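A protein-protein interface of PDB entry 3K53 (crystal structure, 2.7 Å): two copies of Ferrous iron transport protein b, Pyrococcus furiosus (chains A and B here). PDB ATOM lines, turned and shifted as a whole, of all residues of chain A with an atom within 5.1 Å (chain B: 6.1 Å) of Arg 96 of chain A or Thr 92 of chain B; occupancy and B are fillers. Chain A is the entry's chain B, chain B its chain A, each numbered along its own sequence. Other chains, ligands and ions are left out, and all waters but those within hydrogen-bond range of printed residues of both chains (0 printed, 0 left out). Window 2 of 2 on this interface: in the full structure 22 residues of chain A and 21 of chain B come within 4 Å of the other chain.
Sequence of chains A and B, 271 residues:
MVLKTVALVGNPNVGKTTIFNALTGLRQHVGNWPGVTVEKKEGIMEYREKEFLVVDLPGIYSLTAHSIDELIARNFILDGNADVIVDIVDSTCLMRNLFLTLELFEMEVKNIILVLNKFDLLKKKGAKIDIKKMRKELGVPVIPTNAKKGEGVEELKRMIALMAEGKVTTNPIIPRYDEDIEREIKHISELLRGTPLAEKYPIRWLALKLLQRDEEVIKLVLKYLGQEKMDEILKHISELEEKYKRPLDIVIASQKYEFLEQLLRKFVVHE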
ATOM      1  N   ASN A  11      16.269  -5.305   3.407  1.00  0.00           N
ATOM      2  CA  ASN A  11      14.911  -4.810   3.195  1.00  0.00           C
ATOM      3  C   ASN A  11      14.722  -4.304   1.768  1.00  0.00           C
ATOM      4  O   ASN A  11      15.677  -4.178   0.999  1.00  0.00           O
ATOM      5  CB  ASN A  11      14.595  -3.649   4.134  1.00  0.00           C
ATOM      6  CG  ASN A  11      14.711  -4.020   5.584  1.00  0.00           C
ATOM      7  OD1 ASN A  11      14.335  -5.128   5.984  1.00  0.00           O
ATOM      8  ND2 ASN A  11      15.216  -3.086   6.395  1.00  0.00           N
ATOM      9  N   TYR A  61      11.605  -7.921   5.601  1.00  0.00           N
ATOM     10  CA  TYR A  61      11.739  -7.199   6.869  1.00  0.00           C
ATOM     11  C   TYR A  61      12.101  -8.090   8.058  1.00  0.00           C
ATOM     12  O   TYR A  61      12.655  -7.619   9.055  1.00  0.00           O
ATOM     13  CB  TYR A  61      10.460  -6.404   7.147  1.00  0.00           C
ATOM     14  CG  TYR A  61      10.369  -5.176   6.275  1.00  0.00           C
ATOM     15  CD1 TYR A  61      11.335  -4.171   6.372  1.00  0.00           C
ATOM     16  CD2 TYR A  61       9.364  -5.038   5.312  1.00  0.00           C
ATOM     17  CE1 TYR A  61      11.315  -3.058   5.532  1.00  0.00           C
ATOM     18  CE2 TYR A  61       9.329  -3.925   4.458  1.00  0.00           C
ATOM     19  CZ  TYR A  61      10.314  -2.942   4.575  1.00  0.00           C
ATOM     20  OH  TYR A  61      10.341  -1.862   3.721  1.00  0.00           O
ATOM     21  N   CYS A  93      17.946   3.941   8.446  1.00  0.00           N
ATOM     22  CA  CYS A  93      17.007   3.419   9.441  1.00  0.00           C
ATOM     23  C   CYS A  93      17.621   2.163  10.036  1.00  0.00           C
ATOM     24  O   CYS A  93      17.111   1.053   9.887  1.00  0.00           O
ATOM     25  CB  CYS A  93      15.638   3.120   8.806  1.00  0.00           C
ATOM     26  SG  CYS A  93      14.278   2.769   9.984  1.00  0.00           S
ATOM     27  N   LEU A  94      18.743   2.358  10.718  1.00  0.00           N
ATOM     28  CA  LEU A  94      19.448   1.253  11.325  1.00  0.00           C
ATOM     29  C   LEU A  94      18.601   0.356  12.218  1.00  0.00           C
ATOM     30  O   LEU A  94      18.717  -0.868  12.127  1.00  0.00           O
ATOM     31  CB  LEU A  94      20.663   1.769  12.087  1.00  0.00           C
ATOM     32  CG  LEU A  94      21.844   2.093  11.174  1.00  0.00           C
ATOM     33  CD1 LEU A  94      23.043   2.484  11.996  1.00  0.00           C
ATOM     34  CD2 LEU A  94      22.187   0.870  10.340  1.00  0.00           C
ATOM     35  N   MET A  95      17.741   0.935  13.057  1.00  0.00           N
ATOM     36  CA  MET A  95      16.927   0.105  13.942  1.00  0.00           C
ATOM     37  C   MET A  95      16.125  -0.954  13.192  1.00  0.00           C
ATOM     38  O   MET A  95      16.262  -2.150  13.475  1.00  0.00           O
ATOM     39  CB  MET A  95      15.978   0.941  14.807  1.00  0.00           C
ATOM     40  CG  MET A  95      15.159   0.052  15.768  1.00  0.00           C
ATOM     41  SD  MET A  95      14.384   0.833  17.211  1.00  0.00           S
ATOM     42  CE  MET A  95      15.710   0.694  18.414  1.00  0.00           C
ATOM     43  N   ARG A  96      15.301  -0.525  12.240  1.00  0.00           N
ATOM     44  CA  ARG A  96      14.495  -1.460  11.466  1.00  0.00           C
ATOM     45  C   ARG A  96      15.334  -2.458  10.668  1.00  0.00           C
ATOM     46  O   ARG A  96      15.011  -3.652  10.621  1.00  0.00           O
ATOM     47  CB  ARG A  96      13.561  -0.701  10.514  1.00  0.00           C
ATOM     48  CG  ARG A  96      12.997  -1.551   9.376  1.00  0.00           C
ATOM     49  CD  ARG A  96      11.613  -1.091   8.926  1.00  0.00           C
ATOM     50  NE  ARG A  96      11.555   0.340   8.612  1.00  0.00           N
ATOM     51  CZ  ARG A  96      12.119   0.917   7.553  1.00  0.00           C
ATOM     52  NH1 ARG A  96      12.801   0.194   6.667  1.00  0.00           N
ATOM     53  NH2 ARG A  96      11.999   2.224   7.384  1.00  0.00           N
ATOM     54  N   ASN A  97      16.408  -1.970  10.050  1.00  0.00           N
ATOM     55  CA  ASN A  97      17.262  -2.825   9.234  1.00  0.00           C
ATOM     56  C   ASN A  97      18.067  -3.858  10.005  1.00  0.00           C
ATOM     57  O   ASN A  97      18.146  -5.017   9.578  1.00  0.00           O
ATOM     58  CB  ASN A  97      18.202  -1.984   8.349  1.00  0.00           C
ATOM     59  CG  ASN A  97      17.517  -1.487   7.077  1.00  0.00           C
ATOM     60  OD1 ASN A  97      16.687  -0.584   7.122  1.00  0.00           O
ATOM     61  ND2 ASN A  97      17.851  -2.091   5.943  1.00  0.00           N
ATOM     62  N   LEU A  98      18.671  -3.457  11.123  1.00  0.00           N
ATOM     63  CA  LEU A  98      19.447  -4.405  11.919  1.00  0.00           C
ATOM     64  C   LEU A  98      18.532  -5.456  12.543  1.00  0.00           C
ATOM     65  O   LEU A  98      19.000  -6.492  13.019  1.00  0.00           O
ATOM     66  CB  LEU A  98      20.219  -3.687  13.015  1.00  0.00           C
ATOM     67  CG  LEU A  98      21.315  -2.757  12.503  1.00  0.00           C
ATOM     68  CD1 LEU A  98      21.902  -2.001  13.669  1.00  0.00           C
ATOM     69  CD2 LEU A  98      22.386  -3.548  11.769  1.00  0.00           C
ATOM     70  N   PHE A  99      17.228  -5.194  12.546  1.00  0.00           N
ATOM     71  CA  PHE A  99      16.292  -6.147  13.115  1.00  0.00           C
ATOM     72  C   PHE A  99      16.391  -7.444  12.307  1.00  0.00           C
ATOM     73  O   PHE A  99      16.347  -8.535  12.863  1.00  0.00           O
ATOM     74  CB  PHE A  99      14.866  -5.599  13.069  1.00  0.00           C
ATOM     75  CG  PHE A  99      13.830  -6.536  13.641  1.00  0.00           C
ATOM     76  CD1 PHE A  99      13.389  -6.392  14.950  1.00  0.00           C
ATOM     77  CD2 PHE A  99      13.307  -7.572  12.870  1.00  0.00           C
ATOM     78  CE1 PHE A  99      12.441  -7.267  15.485  1.00  0.00           C
ATOM     79  CE2 PHE A  99      12.361  -8.452  13.395  1.00  0.00           C
ATOM     80  CZ  PHE A  99      11.928  -8.300  14.702  1.00  0.00           C
ATOM     81  N   LEU A 100      16.532  -7.325  10.991  1.00  0.00           N
ATOM     82  CA  LEU A 100      16.649  -8.506  10.143  1.00  0.00           C
ATOM     83  C   LEU A 100      18.006  -9.142  10.407  1.00  0.00           C
ATOM     84  O   LEU A 100      18.118 -10.357  10.560  1.00  0.00           O
ATOM     85  CB  LEU A 100      16.516  -8.113   8.676  1.00  0.00           C
ATOM     86  CG  LEU A 100      16.650  -9.207   7.627  1.00  0.00           C
ATOM     87  CD1 LEU A 100      15.662 -10.330   7.891  1.00  0.00           C
ATOM     88  CD2 LEU A 100      16.405  -8.591   6.268  1.00  0.00           C
ATOM     89  N   VAL B  89       9.350  13.997  13.585  1.00  0.00           N
ATOM     90  CA  VAL B  89       9.618  12.581  13.385  1.00  0.00           C
ATOM     91  C   VAL B  89       9.863  12.197  11.943  1.00  0.00           C
ATOM     92  O   VAL B  89       9.218  12.718  11.043  1.00  0.00           O
ATOM     93  CB  VAL B  89       8.419  11.765  13.897  1.00  0.00           C
ATOM     94  CG1 VAL B  89       8.522  10.340  13.457  1.00  0.00           C
ATOM     95  CG2 VAL B  89       8.347  11.869  15.416  1.00  0.00           C
ATOM     96  N   ASP B  90      10.793  11.280  11.715  1.00  0.00           N
ATOM     97  CA  ASP B  90      11.040  10.845  10.358  1.00  0.00           C
ATOM     98  C   ASP B  90      10.023   9.761  10.056  1.00  0.00           C
ATOM     99  O   ASP B  90      10.044   8.699  10.675  1.00  0.00           O
ATOM    100  CB  ASP B  90      12.435  10.275  10.205  1.00  0.00           C
ATOM    101  CG  ASP B  90      12.747   9.930   8.768  1.00  0.00           C
ATOM    102  OD1 ASP B  90      11.857   9.342   8.105  1.00  0.00           O
ATOM    103  OD2 ASP B  90      13.872  10.244   8.306  1.00  0.00           O
ATOM    104  N   SER B  91       9.136  10.030   9.102  1.00  0.00           N
ATOM    105  CA  SER B  91       8.084   9.083   8.729  1.00  0.00           C
ATOM    106  C   SER B  91       8.588   7.744   8.210  1.00  0.00           C
ATOM    107  O   SER B  91       7.870   6.747   8.269  1.00  0.00           O
ATOM    108  CB  SER B  91       7.155   9.711   7.684  1.00  0.00           C
ATOM    109  OG  SER B  91       6.358  10.724   8.272  1.00  0.00           O
ATOM    110  N   THR B  92       9.821   7.715   7.719  1.00  0.00           N
ATOM    111  CA  THR B  92      10.375   6.485   7.182  1.00  0.00           C
ATOM    112  C   THR B  92      11.065   5.575   8.204  1.00  0.00           C
ATOM    113  O   THR B  92      11.628   4.546   7.837  1.00  0.00           O
ATOM    114  CB  THR B  92      11.379   6.783   6.047  1.00  0.00           C
ATOM    115  OG1 THR B  92      12.417   7.642   6.530  1.00  0.00           O
ATOM    116  CG2 THR B  92      10.679   7.438   4.880  1.00  0.00           C
ATOM    117  N   CYS B  93      11.021   5.938   9.480  1.00  0.00           N
ATOM    118  CA  CYS B  93      11.668   5.130  10.504  1.00  0.00           C
ATOM    119  C   CYS B  93      10.930   5.349  11.837  1.00  0.00           C
ATOM    120  O   CYS B  93      11.522   5.768  12.836  1.00  0.00           O
ATOM    121  CB  CYS B  93      13.134   5.551  10.589  1.00  0.00           C
ATOM    122  SG  CYS B  93      14.283   4.333  11.300  1.00  0.00           S
ATOM    123  N   LEU B  94       9.631   5.048  11.842  1.00  0.00           N
ATOM    124  CA  LEU B  94       8.789   5.252  13.018  1.00  0.00           C
ATOM    125  C   LEU B  94       9.194   4.629  14.337  1.00  0.00           C
ATOM    126  O   LEU B  94       9.259   5.343  15.331  1.00  0.00           O
ATOM    127  CB  LEU B  94       7.342   4.881  12.702  1.00  0.00           C
ATOM    128  CG  LEU B  94       6.710   5.963  11.823  1.00  0.00           C
ATOM    129  CD1 LEU B  94       5.349   5.513  11.323  1.00  0.00           C
ATOM    130  CD2 LEU B  94       6.601   7.257  12.613  1.00  0.00           C
ATOM    131  N   MET B  95       9.454   3.322  14.367  1.00  0.00           N
ATOM    132  CA  MET B  95       9.857   2.644  15.607  1.00  0.00           C
ATOM    133  C   MET B  95      10.931   3.453  16.350  1.00  0.00           C
ATOM    134  O   MET B  95      10.695   3.905  17.468  1.00  0.00           O
ATOM    135  CB  MET B  95      10.391   1.246  15.298  1.00  0.00           C
ATOM    136  CG  MET B  95      10.507   0.314  16.495  1.00  0.00           C
ATOM    137  SD  MET B  95       9.035  -0.705  16.693  1.00  0.00           S
ATOM    138  CE  MET B  95       8.232   0.160  17.903  1.00  0.00           C
ATOM    139  N   ASN B 117       7.454  14.068   9.298  1.00  0.00           N
ATOM    140  CA  ASN B 117       8.229  14.644   8.216  1.00  0.00           C
ATOM    141  C   ASN B 117       8.750  13.605   7.250  1.00  0.00           C
ATOM    142  O   ASN B 117       8.778  12.421   7.553  1.00  0.00           O
ATOM    143  CB  ASN B 117       9.401  15.429   8.752  1.00  0.00           C
ATOM    144  CG  ASN B 117      10.057  16.244   7.682  1.00  0.00           C
ATOM    145  OD1 ASN B 117      11.271  16.402   7.667  1.00  0.00           O
ATOM    146  ND2 ASN B 117       9.251  16.780   6.772  1.00  0.00           N
ATOM    147  N   LYS B 118       9.207  14.069   6.095  1.00  0.00           N
ATOM    148  CA  LYS B 118       9.689  13.183   5.036  1.00  0.00           C
ATOM    149  C   LYS B 118       8.545  12.264   4.626  1.00  0.00           C
ATOM    150  O   LYS B 118       8.746  11.087   4.358  1.00  0.00           O
ATOM    151  CB  LYS B 118      10.899  12.367   5.493  1.00  0.00           C
ATOM    152  CG  LYS B 118      12.196  13.152   5.395  1.00  0.00           C
ATOM    153  CD  LYS B 118      13.392  12.439   6.042  1.00  0.00           C
ATOM    154  CE  LYS B 118      14.579  13.395   6.140  1.00  0.00           C
ATOM    155  NZ  LYS B 118      15.662  12.901   7.039  1.00  0.00           N
ATOM    156  N   LEU B 121       8.968  10.714   1.010  1.00  0.00           N
ATOM    157  CA  LEU B 121       9.756   9.490   0.930  1.00  0.00           C
ATOM    158  C   LEU B 121       8.958   8.293   1.440  1.00  0.00           C
ATOM    159  O   LEU B 121       9.287   7.143   1.161  1.00  0.00           O
ATOM    160  CB  LEU B 121      11.040   9.642   1.746  1.00  0.00           C
ATOM    161  CG  LEU B 121      11.894  10.878   1.442  1.00  0.00           C
ATOM    162  CD1 LEU B 121      13.109  10.876   2.344  1.00  0.00           C
ATOM    163  CD2 LEU B 121      12.321  10.888  -0.018  1.00  0.00           C
ATOM    164  N   LEU B 122       7.905   8.579   2.194  1.00  0.00           N
ATOM    165  CA  LEU B 122       7.044   7.543   2.754  1.00  0.00           C
ATOM    166  C   LEU B 122       6.240   6.866   1.657  1.00  0.00           C
ATOM    167  O   LEU B 122       6.541   5.739   1.250  1.00  0.00           O
ATOM    168  CB  LEU B 122       6.068   8.153   3.762  1.00  0.00           C
ATOM    169  CG  LEU B 122       5.047   7.182   4.348  1.00  0.00           C
ATOM    170  CD1 LEU B 122       5.716   6.360   5.429  1.00  0.00           C
ATOM    171  CD2 LEU B 122       3.872   7.951   4.913  1.00  0.00           C
ATOM    172  N   LYS B 125       8.401   4.820  -1.184  1.00  0.00           N
ATOM    173  CA  LYS B 125       8.830   3.441  -0.995  1.00  0.00           C
ATOM    174  C   LYS B 125       7.589   2.552  -0.937  1.00  0.00           C
ATOM    175  O   LYS B 125       7.687   1.326  -0.960  1.00  0.00           O
ATOM    176  CB  LYS B 125       9.652   3.305   0.301  1.00  0.00           C
ATOM    177  CG  LYS B 125       8.857   3.013   1.589  1.00  0.00           C
ATOM    178  CD  LYS B 125       8.772   1.510   1.874  1.00  0.00           C
ATOM    179  CE  LYS B 125       8.044   1.202   3.186  1.00  0.00           C
ATOM    180  NZ  LYS B 125       8.787   1.643   4.406  1.00  0.00           N
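NH2 of Arg 96 of chain A sits close to O of Thr 92 of chain B (2.4 Å). The side-chain sulfur (SG) of Cys 93 of chain A is disulfide-bonded to the side-chain sulfur (SG) of Cys 93 of chain B, 2.0 Å away.
The side-chain sulfur (SG) of Cys 93 of chain A is in hydrogen-bond range of the guanidinium group (NH2) of Arg 96 of chain A (3.5 Å). The side-chain carboxylate (OD1) of Asp 90 of chain B sits at hydrogen-bond distance from the backbone NH (N) of Thr 92 of chain B (2.6 Å). O of Cys 93 of chain A sits close to OD1 of Asn 97 of chain A, at 3.2 Å.
Lys 125 of chain B touches Tyr 61 of chain A. Thr 92 of chain B touches Cys 93 of chain A (O to SG, 3.8 Å). Met 95 of chain B touches Met 95 of chain A.
Printed residues of chain B within 4 Å of Tyr 61 of chain A: Lys 125. Of the printed residues of chain B, Met 95 of chain A touches Met 95. Arg 96 of chain A touches just one residue of chain B: Thr 92 (2.4 Å). Of chain A, only Cys 93 and Arg 96 come within 4 Å of Thr 92 of chain B. Of the printed residues of chain A, Cys 93 of chain B touches Cys 93 (2.0 Å). Leu 94 of chain B touches none of the printed residues of chain A. Of the printed residues of chain A, Met 95 of chain B touches Met 95. Printed residues of chain A within 4 Å of Lys 125 of chain B: Tyr 61 (3.9 Å). The nearest residue of chain B that does not touch Arg 96 of chain A is Cys 93 of chain B (4.3 Å).
Of the 12 printed residues of chain B, 4 touch a printed residue of chain A. Hydrophobic or aromatic side chains of chain B within 4 Å of the printed part of chain A: Met 95. Printed residues of chain A that touch a printed residue of chain B: Tyr 61, Cys 93, Met 95 and Arg 96. Hydrophobic or aromatic side chains of chain A that line the printed part of chain B: Tyr 61 and Met 95. Among the printed residues, 5 pairs touch across the chains. Among the printed residues, no Asp or Glu carboxylate lies within 4 Å of a Lys or Arg side-chain nitrogen of the other chain.
Cys 93 of chain B touches its own counterpart, Cys 93 of chain A. Met 95 of chain B touches its own counterpart, Met 95 of chain A.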
